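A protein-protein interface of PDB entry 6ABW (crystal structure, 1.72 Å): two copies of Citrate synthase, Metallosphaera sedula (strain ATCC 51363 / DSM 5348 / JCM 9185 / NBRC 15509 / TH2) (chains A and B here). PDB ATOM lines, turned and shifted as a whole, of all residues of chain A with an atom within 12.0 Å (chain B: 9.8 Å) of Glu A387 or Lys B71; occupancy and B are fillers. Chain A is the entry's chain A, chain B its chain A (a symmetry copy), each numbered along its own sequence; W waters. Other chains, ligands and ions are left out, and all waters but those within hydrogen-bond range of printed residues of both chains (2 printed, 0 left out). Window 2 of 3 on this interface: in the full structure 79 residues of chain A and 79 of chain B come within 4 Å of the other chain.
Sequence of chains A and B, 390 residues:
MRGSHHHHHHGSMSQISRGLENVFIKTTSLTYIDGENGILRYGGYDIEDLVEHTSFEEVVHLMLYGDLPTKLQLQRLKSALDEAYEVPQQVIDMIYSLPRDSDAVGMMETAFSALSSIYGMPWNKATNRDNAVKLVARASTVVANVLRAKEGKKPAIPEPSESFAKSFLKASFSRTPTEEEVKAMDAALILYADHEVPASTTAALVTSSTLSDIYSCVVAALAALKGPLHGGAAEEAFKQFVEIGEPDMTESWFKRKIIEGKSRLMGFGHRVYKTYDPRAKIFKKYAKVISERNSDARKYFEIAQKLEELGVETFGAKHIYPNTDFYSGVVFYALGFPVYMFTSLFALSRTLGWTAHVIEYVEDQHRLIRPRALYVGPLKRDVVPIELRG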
ATOM      1  N   ASP A 382      -1.510 -18.985  35.821  1.00  0.00           N
ATOM      2  CA  ASP A 382      -2.615 -18.634  34.980  1.00  0.00           C
ATOM      3  C   ASP A 382      -2.058 -17.850  33.802  1.00  0.00           C
ATOM      4  O   ASP A 382      -1.132 -17.062  33.982  1.00  0.00           O
ATOM      5  CB  ASP A 382      -3.648 -17.752  35.739  1.00  0.00           C
ATOM      6  CG  ASP A 382      -4.385 -18.500  36.861  1.00  0.00           C
ATOM      7  OD1 ASP A 382      -4.363 -19.746  36.933  1.00  0.00           O
ATOM      8  OD2 ASP A 382      -5.041 -17.809  37.666  1.00  0.00           O
ATOM      9  N   VAL A 383      -2.659 -18.018  32.632  1.00  0.00           N
ATOM     10  CA  VAL A 383      -2.216 -17.285  31.461  1.00  0.00           C
ATOM     11  C   VAL A 383      -2.607 -15.822  31.710  1.00  0.00           C
ATOM     12  O   VAL A 383      -3.729 -15.526  32.118  1.00  0.00           O
ATOM     13  CB  VAL A 383      -2.872 -17.732  30.131  1.00  0.00           C
ATOM     14  CG1 VAL A 383      -2.592 -16.745  28.994  1.00  0.00           C
ATOM     15  CG2 VAL A 383      -2.420 -19.135  29.716  1.00  0.00           C
ATOM     16  N   VAL A 384      -1.694 -14.940  31.351  1.00  0.00           N
ATOM     17  CA  VAL A 384      -1.910 -13.505  31.420  1.00  0.00           C
ATOM     18  C   VAL A 384      -1.916 -12.964  29.989  1.00  0.00           C
ATOM     19  O   VAL A 384      -1.120 -13.401  29.147  1.00  0.00           O
ATOM     20  CB  VAL A 384      -0.822 -12.985  32.387  1.00  0.00           C
ATOM     21  CG1 VAL A 384       0.010 -11.863  31.839  1.00  0.00           C
ATOM     22  CG2 VAL A 384      -1.442 -12.740  33.757  1.00  0.00           C
ATOM     23  N   PRO A 385      -2.805 -12.030  29.691  1.00  0.00           N
ATOM     24  CA  PRO A 385      -2.821 -11.396  28.360  1.00  0.00           C
ATOM     25  C   PRO A 385      -1.476 -10.788  27.962  1.00  0.00           C
ATOM     26  O   PRO A 385      -0.777 -10.248  28.800  1.00  0.00           O
ATOM     27  CB  PRO A 385      -3.870 -10.283  28.496  1.00  0.00           C
ATOM     28  CG  PRO A 385      -4.642 -10.615  29.737  1.00  0.00           C
ATOM     29  CD  PRO A 385      -3.763 -11.402  30.622  1.00  0.00           C
ATOM     30  N   ILE A 386      -1.146 -10.848  26.683  1.00  0.00           N
ATOM     31  CA  ILE A 386       0.187 -10.490  26.231  1.00  0.00           C
ATOM     32  C   ILE A 386       0.610  -9.053  26.641  1.00  0.00           C
ATOM     33  O   ILE A 386       1.759  -8.854  27.027  1.00  0.00           O
ATOM     34  CB  ILE A 386       0.350 -10.749  24.700  1.00  0.00           C
ATOM     35  CG1 ILE A 386       1.835 -10.780  24.306  1.00  0.00           C
ATOM     36  CG2 ILE A 386      -0.495  -9.800  23.889  1.00  0.00           C
ATOM     37  CD1 ILE A 386       2.059 -11.124  22.802  1.00  0.00           C
ATOM     38  N   GLU A 387      -0.341  -8.133  26.660  1.00  0.00           N
ATOM     39  CA  GLU A 387      -0.089  -6.705  27.066  1.00  0.00           C
ATOM     40  C   GLU A 387       0.456  -6.583  28.500  1.00  0.00           C
ATOM     41  O   GLU A 387       1.243  -5.696  28.795  1.00  0.00           O
ATOM     42  CB  GLU A 387      -1.387  -5.892  26.940  1.00  0.00           C
ATOM     43  CG  GLU A 387      -1.936  -5.691  25.515  1.00  0.00           C
ATOM     44  CD  GLU A 387      -2.683  -6.905  24.892  1.00  0.00           C
ATOM     45  OE1 GLU A 387      -2.778  -6.881  23.615  1.00  0.00           O
ATOM     46  OE2 GLU A 387      -3.146  -7.879  25.627  1.00  0.00           O
ATOM     47  N   LEU A 388       0.073  -7.518  29.366  1.00  0.00           N
ATOM     48  CA  LEU A 388       0.578  -7.590  30.725  1.00  0.00           C
ATOM     49  C   LEU A 388       1.844  -8.347  30.938  1.00  0.00           C
ATOM     50  O   LEU A 388       2.314  -8.502  32.094  1.00  0.00           O
ATOM     51  CB  LEU A 388      -0.497  -8.165  31.622  1.00  0.00           C
ATOM     52  CG  LEU A 388      -1.762  -7.363  31.772  1.00  0.00           C
ATOM     53  CD1 LEU A 388      -2.827  -8.234  32.405  1.00  0.00           C
ATOM     54  CD2 LEU A 388      -1.527  -6.200  32.680  1.00  0.00           C
ATOM     55  N   ARG A 389       2.446  -8.865  29.861  1.00  0.00           N
ATOM     56  CA  ARG A 389       3.681  -9.566  30.021  1.00  0.00           C
ATOM     57  C   ARG A 389       4.822  -8.551  29.920  1.00  0.00           C
ATOM     58  O   ARG A 389       5.922  -8.955  30.092  1.00  0.00           O
ATOM     59  CB  ARG A 389       3.784 -10.707  28.970  1.00  0.00           C
ATOM     60  CG  ARG A 389       2.647 -11.747  29.084  1.00  0.00           C
ATOM     61  CD  ARG A 389       2.705 -12.801  27.957  1.00  0.00           C
ATOM     62  NE  ARG A 389       1.417 -13.454  27.792  1.00  0.00           N
ATOM     63  CZ  ARG A 389       0.989 -14.008  26.671  1.00  0.00           C
ATOM     64  NH1 ARG A 389       1.810 -14.098  25.583  1.00  0.00           N
ATOM     65  NH2 ARG A 389      -0.227 -14.524  26.661  1.00  0.00           N
ATOM     66  N   HIS B  53      -6.718 -19.183  25.273  1.00  0.00           N
ATOM     67  CA  HIS B  53      -6.177 -17.838  25.427  1.00  0.00           C
ATOM     68  C   HIS B  53      -4.829 -17.598  24.736  1.00  0.00           C
ATOM     69  O   HIS B  53      -4.339 -16.449  24.751  1.00  0.00           O
ATOM     70  CB  HIS B  53      -6.047 -17.515  26.898  1.00  0.00           C
ATOM     71  CG  HIS B  53      -7.346 -17.536  27.631  1.00  0.00           C
ATOM     72  ND1 HIS B  53      -7.578 -18.364  28.713  1.00  0.00           N
ATOM     73  CD2 HIS B  53      -8.462 -16.779  27.487  1.00  0.00           C
ATOM     74  CE1 HIS B  53      -8.805 -18.140  29.176  1.00  0.00           C
ATOM     75  NE2 HIS B  53      -9.358 -17.178  28.454  1.00  0.00           N
ATOM     76  N   GLU B  58       2.768 -18.947  20.491  1.00  0.00           N
ATOM     77  CA  GLU B  58       3.008 -18.707  21.898  1.00  0.00           C
ATOM     78  C   GLU B  58       3.417 -19.920  22.682  1.00  0.00           C
ATOM     79  O   GLU B  58       4.273 -19.834  23.515  1.00  0.00           O
ATOM     80  CB  GLU B  58       1.794 -17.993  22.556  1.00  0.00           C
ATOM     81  CG  GLU B  58       1.608 -16.547  22.086  1.00  0.00           C
ATOM     82  CD  GLU B  58       0.252 -15.937  22.524  1.00  0.00           C
ATOM     83  OE1 GLU B  58       0.251 -15.134  23.508  1.00  0.00           O
ATOM     84  OE2 GLU B  58      -0.827 -16.315  21.965  1.00  0.00           O
ATOM     85  N   HIS B  61       7.051 -20.721  21.925  1.00  0.00           N
ATOM     86  CA  HIS B  61       7.904 -19.891  22.803  1.00  0.00           C
ATOM     87  C   HIS B  61       7.940 -20.406  24.227  1.00  0.00           C
ATOM     88  O   HIS B  61       9.005 -20.507  24.813  1.00  0.00           O
ATOM     89  CB  HIS B  61       7.455 -18.417  22.697  1.00  0.00           C
ATOM     90  CG  HIS B  61       8.416 -17.456  23.300  1.00  0.00           C
ATOM     91  ND1 HIS B  61       8.639 -17.369  24.652  1.00  0.00           N
ATOM     92  CD2 HIS B  61       9.345 -16.653  22.709  1.00  0.00           C
ATOM     93  CE1 HIS B  61       9.614 -16.505  24.885  1.00  0.00           C
ATOM     94  NE2 HIS B  61      10.066 -16.066  23.720  1.00  0.00           N
ATOM     95  N   LEU B  68       5.558 -17.676  28.328  1.00  0.00           N
ATOM     96  CA  LEU B  68       4.802 -17.112  27.271  1.00  0.00           C
ATOM     97  C   LEU B  68       5.470 -15.811  26.836  1.00  0.00           C
ATOM     98  O   LEU B  68       6.127 -15.172  27.637  1.00  0.00           O
ATOM     99  CB  LEU B  68       3.356 -16.857  27.636  1.00  0.00           C
ATOM    100  CG  LEU B  68       2.591 -18.163  27.899  1.00  0.00           C
ATOM    101  CD1 LEU B  68       1.343 -17.911  28.683  1.00  0.00           C
ATOM    102  CD2 LEU B  68       2.287 -18.845  26.571  1.00  0.00           C
ATOM    103  N   PRO B  69       5.398 -15.486  25.537  1.00  0.00           N
ATOM    104  CA  PRO B  69       6.202 -14.366  25.100  1.00  0.00           C
ATOM    105  C   PRO B  69       5.566 -13.002  25.327  1.00  0.00           C
ATOM    106  O   PRO B  69       4.339 -12.855  25.262  1.00  0.00           O
ATOM    107  CB  PRO B  69       6.282 -14.589  23.572  1.00  0.00           C
ATOM    108  CG  PRO B  69       4.980 -15.274  23.239  1.00  0.00           C
ATOM    109  CD  PRO B  69       4.711 -16.139  24.437  1.00  0.00           C
ATOM    110  N   THR B  70       6.427 -11.973  25.420  1.00  0.00           N
ATOM    111  CA  THR B  70       5.989 -10.593  25.211  1.00  0.00           C
ATOM    112  C   THR B  70       5.666 -10.316  23.784  1.00  0.00           C
ATOM    113  O   THR B  70       6.047 -11.106  22.889  1.00  0.00           O
ATOM    114  CB  THR B  70       7.095  -9.598  25.600  1.00  0.00           C
ATOM    115  OG1 THR B  70       8.232  -9.770  24.752  1.00  0.00           O
ATOM    116  CG2 THR B  70       7.539  -9.825  26.987  1.00  0.00           C
ATOM    117  N   LYS B  71       5.003  -9.188  23.525  1.00  0.00           N
ATOM    118  CA  LYS B  71       4.729  -8.749  22.135  1.00  0.00           C
ATOM    119  C   LYS B  71       5.976  -8.793  21.229  1.00  0.00           C
ATOM    120  O   LYS B  71       5.922  -9.259  20.095  1.00  0.00           O
ATOM    121  CB  LYS B  71       4.215  -7.320  22.099  1.00  0.00           C
ATOM    122  CG  LYS B  71       2.746  -7.110  22.362  1.00  0.00           C
ATOM    123  CD  LYS B  71       2.450  -5.603  22.430  1.00  0.00           C
ATOM    124  CE  LYS B  71       1.199  -5.306  23.244  1.00  0.00           C
ATOM    125  NZ  LYS B  71      -0.014  -5.813  22.539  1.00  0.00           N
ATOM    126  N   LEU B  72       7.087  -8.291  21.731  1.00  0.00           N
ATOM    127  CA  LEU B  72       8.291  -8.156  20.911  1.00  0.00           C
ATOM    128  C   LEU B  72       8.899  -9.566  20.685  1.00  0.00           C
ATOM    129  O   LEU B  72       9.413  -9.864  19.587  1.00  0.00           O
ATOM    130  CB  LEU B  72       9.299  -7.246  21.592  1.00  0.00           C
ATOM    131  CG  LEU B  72      10.569  -6.921  20.777  1.00  0.00           C
ATOM    132  CD1 LEU B  72      10.250  -5.989  19.612  1.00  0.00           C
ATOM    133  CD2 LEU B  72      11.661  -6.296  21.660  1.00  0.00           C
ATOM    134  N   GLN B  73       8.864 -10.384  21.724  1.00  0.00           N
ATOM    135  CA  GLN B  73       9.324 -11.768  21.599  1.00  0.00           C
ATOM    136  C   GLN B  73       8.491 -12.502  20.568  1.00  0.00           C
ATOM    137  O   GLN B  73       9.045 -13.228  19.690  1.00  0.00           O
ATOM    138  CB  GLN B  73       9.356 -12.512  22.898  1.00  0.00           C
ATOM    139  CG  GLN B  73      10.452 -12.084  23.814  1.00  0.00           C
ATOM    140  CD  GLN B  73      10.339 -12.625  25.218  1.00  0.00           C
ATOM    141  OE1 GLN B  73       9.263 -12.959  25.731  1.00  0.00           O
ATOM    142  NE2 GLN B  73      11.454 -12.644  25.869  1.00  0.00           N
ATOM    143  N   LEU B  74       7.191 -12.313  20.616  1.00  0.00           N
ATOM    144  CA  LEU B  74       6.295 -12.990  19.700  1.00  0.00           C
ATOM    145  C   LEU B  74       6.540 -12.572  18.275  1.00  0.00           C
ATOM    146  O   LEU B  74       6.526 -13.358  17.350  1.00  0.00           O
ATOM    147  CB  LEU B  74       4.857 -12.732  20.042  1.00  0.00           C
ATOM    148  CG  LEU B  74       3.794 -13.427  19.202  1.00  0.00           C
ATOM    149  CD1 LEU B  74       3.983 -14.953  19.113  1.00  0.00           C
ATOM    150  CD2 LEU B  74       2.448 -13.153  19.797  1.00  0.00           C
ATOM    151  N   GLN B  75       6.709 -11.273  18.089  1.00  0.00           N
ATOM    152  CA  GLN B  75       7.064 -10.736  16.792  1.00  0.00           C
ATOM    153  C   GLN B  75       8.338 -11.304  16.166  1.00  0.00           C
ATOM    154  O   GLN B  75       8.344 -11.576  14.939  1.00  0.00           O
ATOM    155  CB  GLN B  75       7.130  -9.205  16.909  1.00  0.00           C
ATOM    156  CG  GLN B  75       7.477  -8.392  15.699  1.00  0.00           C
ATOM    157  CD  GLN B  75       7.827  -6.941  16.114  1.00  0.00           C
ATOM    158  OE1 GLN B  75       8.706  -6.318  15.502  1.00  0.00           O
ATOM    159  NE2 GLN B  75       7.173  -6.425  17.208  1.00  0.00           N
ATOM    160  N   ARG B  76       9.400 -11.441  16.952  1.00  0.00           N
ATOM    161  CA  ARG B  76      10.660 -11.982  16.452  1.00  0.00           C
ATOM    162  C   ARG B  76      10.474 -13.460  16.081  1.00  0.00           C
ATOM    163  O   ARG B  76      10.980 -13.919  15.060  1.00  0.00           O
ATOM    164  CB  ARG B  76      11.797 -11.862  17.478  1.00  0.00           C
ATOM    165  CG  ARG B  76      12.452 -10.452  17.490  1.00  0.00           C
ATOM    166  CD  ARG B  76      13.574 -10.377  18.526  1.00  0.00           C
ATOM    167  NE  ARG B  76      13.118  -9.740  19.767  1.00  0.00           N
ATOM    168  CZ  ARG B  76      13.145 -10.270  21.002  1.00  0.00           C
ATOM    169  NH1 ARG B  76      13.644 -11.483  21.268  1.00  0.00           N
ATOM    170  NH2 ARG B  76      12.679  -9.549  22.015  1.00  0.00           N
ATOM    171  N   LEU B  77       9.693 -14.168  16.898  1.00  0.00           N
ATOM    172  CA  LEU B  77       9.380 -15.580  16.628  1.00  0.00           C
ATOM    173  C   LEU B  77       8.617 -15.761  15.371  1.00  0.00           C
ATOM    174  O   LEU B  77       8.953 -16.641  14.591  1.00  0.00           O
ATOM    175  CB  LEU B  77       8.620 -16.193  17.798  1.00  0.00           C
ATOM    176  CG  LEU B  77       8.024 -17.600  17.546  1.00  0.00           C
ATOM    177  CD1 LEU B  77       9.152 -18.498  17.258  1.00  0.00           C
ATOM    178  CD2 LEU B  77       7.355 -18.047  18.820  1.00  0.00           C
ATOM    179  N   LYS B  78       7.555 -14.998  15.158  1.00  0.00           N
ATOM    180  CA  LYS B  78       6.841 -15.034  13.934  1.00  0.00           C
ATOM    181  C   LYS B  78       7.659 -14.743  12.678  1.00  0.00           C
ATOM    182  O   LYS B  78       7.476 -15.433  11.667  1.00  0.00           O
ATOM    183  CB  LYS B  78       5.672 -14.094  14.011  1.00  0.00           C
ATOM    184  CG  LYS B  78       4.591 -14.597  14.943  1.00  0.00           C
ATOM    185  CD  LYS B  78       3.489 -13.575  15.030  1.00  0.00           C
ATOM    186  CE  LYS B  78       2.279 -14.193  15.723  1.00  0.00           C
ATOM    187  NZ  LYS B  78       1.252 -13.128  15.808  1.00  0.00           N
ATOM    188  N   SER B  79       8.510 -13.719  12.704  1.00  0.00           N
ATOM    189  CA  SER B  79       9.391 -13.426  11.539  1.00  0.00           C
ATOM    190  C   SER B  79      10.363 -14.605  11.275  1.00  0.00           C
ATOM    191  O   SER B  79      10.646 -14.929  10.117  1.00  0.00           O
ATOM    192  CB  SER B  79      10.279 -12.201  11.805  1.00  0.00           C
ATOM    193  OG  SER B  79       9.454 -11.131  12.094  1.00  0.00           O
HETATM  194  O   HOH W   1      -2.178 -14.870  24.196  1.00  0.00           O
HETATM  195  O   HOH W   2       4.160  -7.831  25.994  1.00  0.00           O
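Of chain B, only Lys B71 (3.2 Å) comes within 4 Å of Glu A387.
Of chain A, only Ile A386 (3.4 Å) and Arg A389 (2.8 Å) come within 4 Å of Pro B69.
Of chain A, only Ile A386 (3.8 Å) and Arg A389 (3.6 Å) come within 4 Å of Thr B70.
No residue of chain A comes within 4 Å of Gln B73.
Leu B74 touches just one residue of chain A: Ile A386.
Printed residues of chain B within 4 Å of Arg A389: Glu B58, Leu B68, Pro B69 and Thr B70.
Printed residues of chain A within 4 Å of Glu B58: Arg A389.
Printed residues of chain A within 4 Å of Leu B68: Arg A389 (3.8 Å).
Asp A382 touches none of the printed residues of chain B.
The nearest residue of chain B that does not touch Glu A387 is Pro B69 (6.8 Å).
The nearest residue of chain A that does not touch Lys B71 is Arg A389 (5.8 Å).
Among the printed residues, merely in contact across the chains: Ile A386 with Pro B69 (3.4 Å), Ile A386 with Lys B71 (3.6 Å), Arg A389 with Thr B70 (3.6 Å), Ile A386 with Leu B74 (3.6 Å), Arg A389 with Leu B68 (3.8 Å) and Ile A386 with Thr B70 (3.8 Å).
Of the 15 printed residues of chain B, 6 touch a printed residue of chain A.
Hydrophobic or aromatic side chains of chain B that line the printed part of chain A: Leu B68, Pro B69 and Leu B74.
Of the 8 printed residues of chain A, 3 touch a printed residue of chain B.
Hydrophobic or aromatic side chains of chain A within 4 Å of the printed part of chain B: Ile A386.
Along chain A the printed residues that touch a printed residue of chain B span positions 386 to 389.
Among the printed residues, Asp or Glu carboxylates within 4 Å of a Lys or Arg side-chain nitrogen of the other chain: Glu A387 with Lys B71 and Arg A389 with Glu B58.
Water W1 lies within hydrogen-bond range of OE1 of Glu B58 (2.5 Å), O of His B53 (2.7 Å) and NH2 of Arg A389 (3.2 Å).
Water W2 lies within hydrogen-bond range of the backbone carbonyl oxygen of Ile A386 (2.8 Å) and the backbone NH of Lys B71 (2.9 Å).
The backbone carbonyl oxygen (O) of Pro B69 is in hydrogen-bond range of the guanidinium group (NH1) of Arg A389 (2.8 Å).
The guanidinium group of Arg A389 is in salt-bridge range of the side-chain carboxylate of Glu B58, at 2.8 Å.
The side-chain carboxylate of Glu A387 lies within salt-bridge range of the side-chain amino group of Lys B71 (3.2 Å).
No position is printed for both chains.
Of the 9 pairs that touch across the chains among the printed residues, none has its exchanged pair printed and touching as well.
The backbone carbonyl oxygen (O) of Val A384 is in hydrogen-bond range of the guanidinium group (NH2) of Arg A389 (2.9 Å).
The side-chain amide oxygen of Gln B73 is in hydrogen-bond range of the backbone NH of Thr B70, at 3.0 Å.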
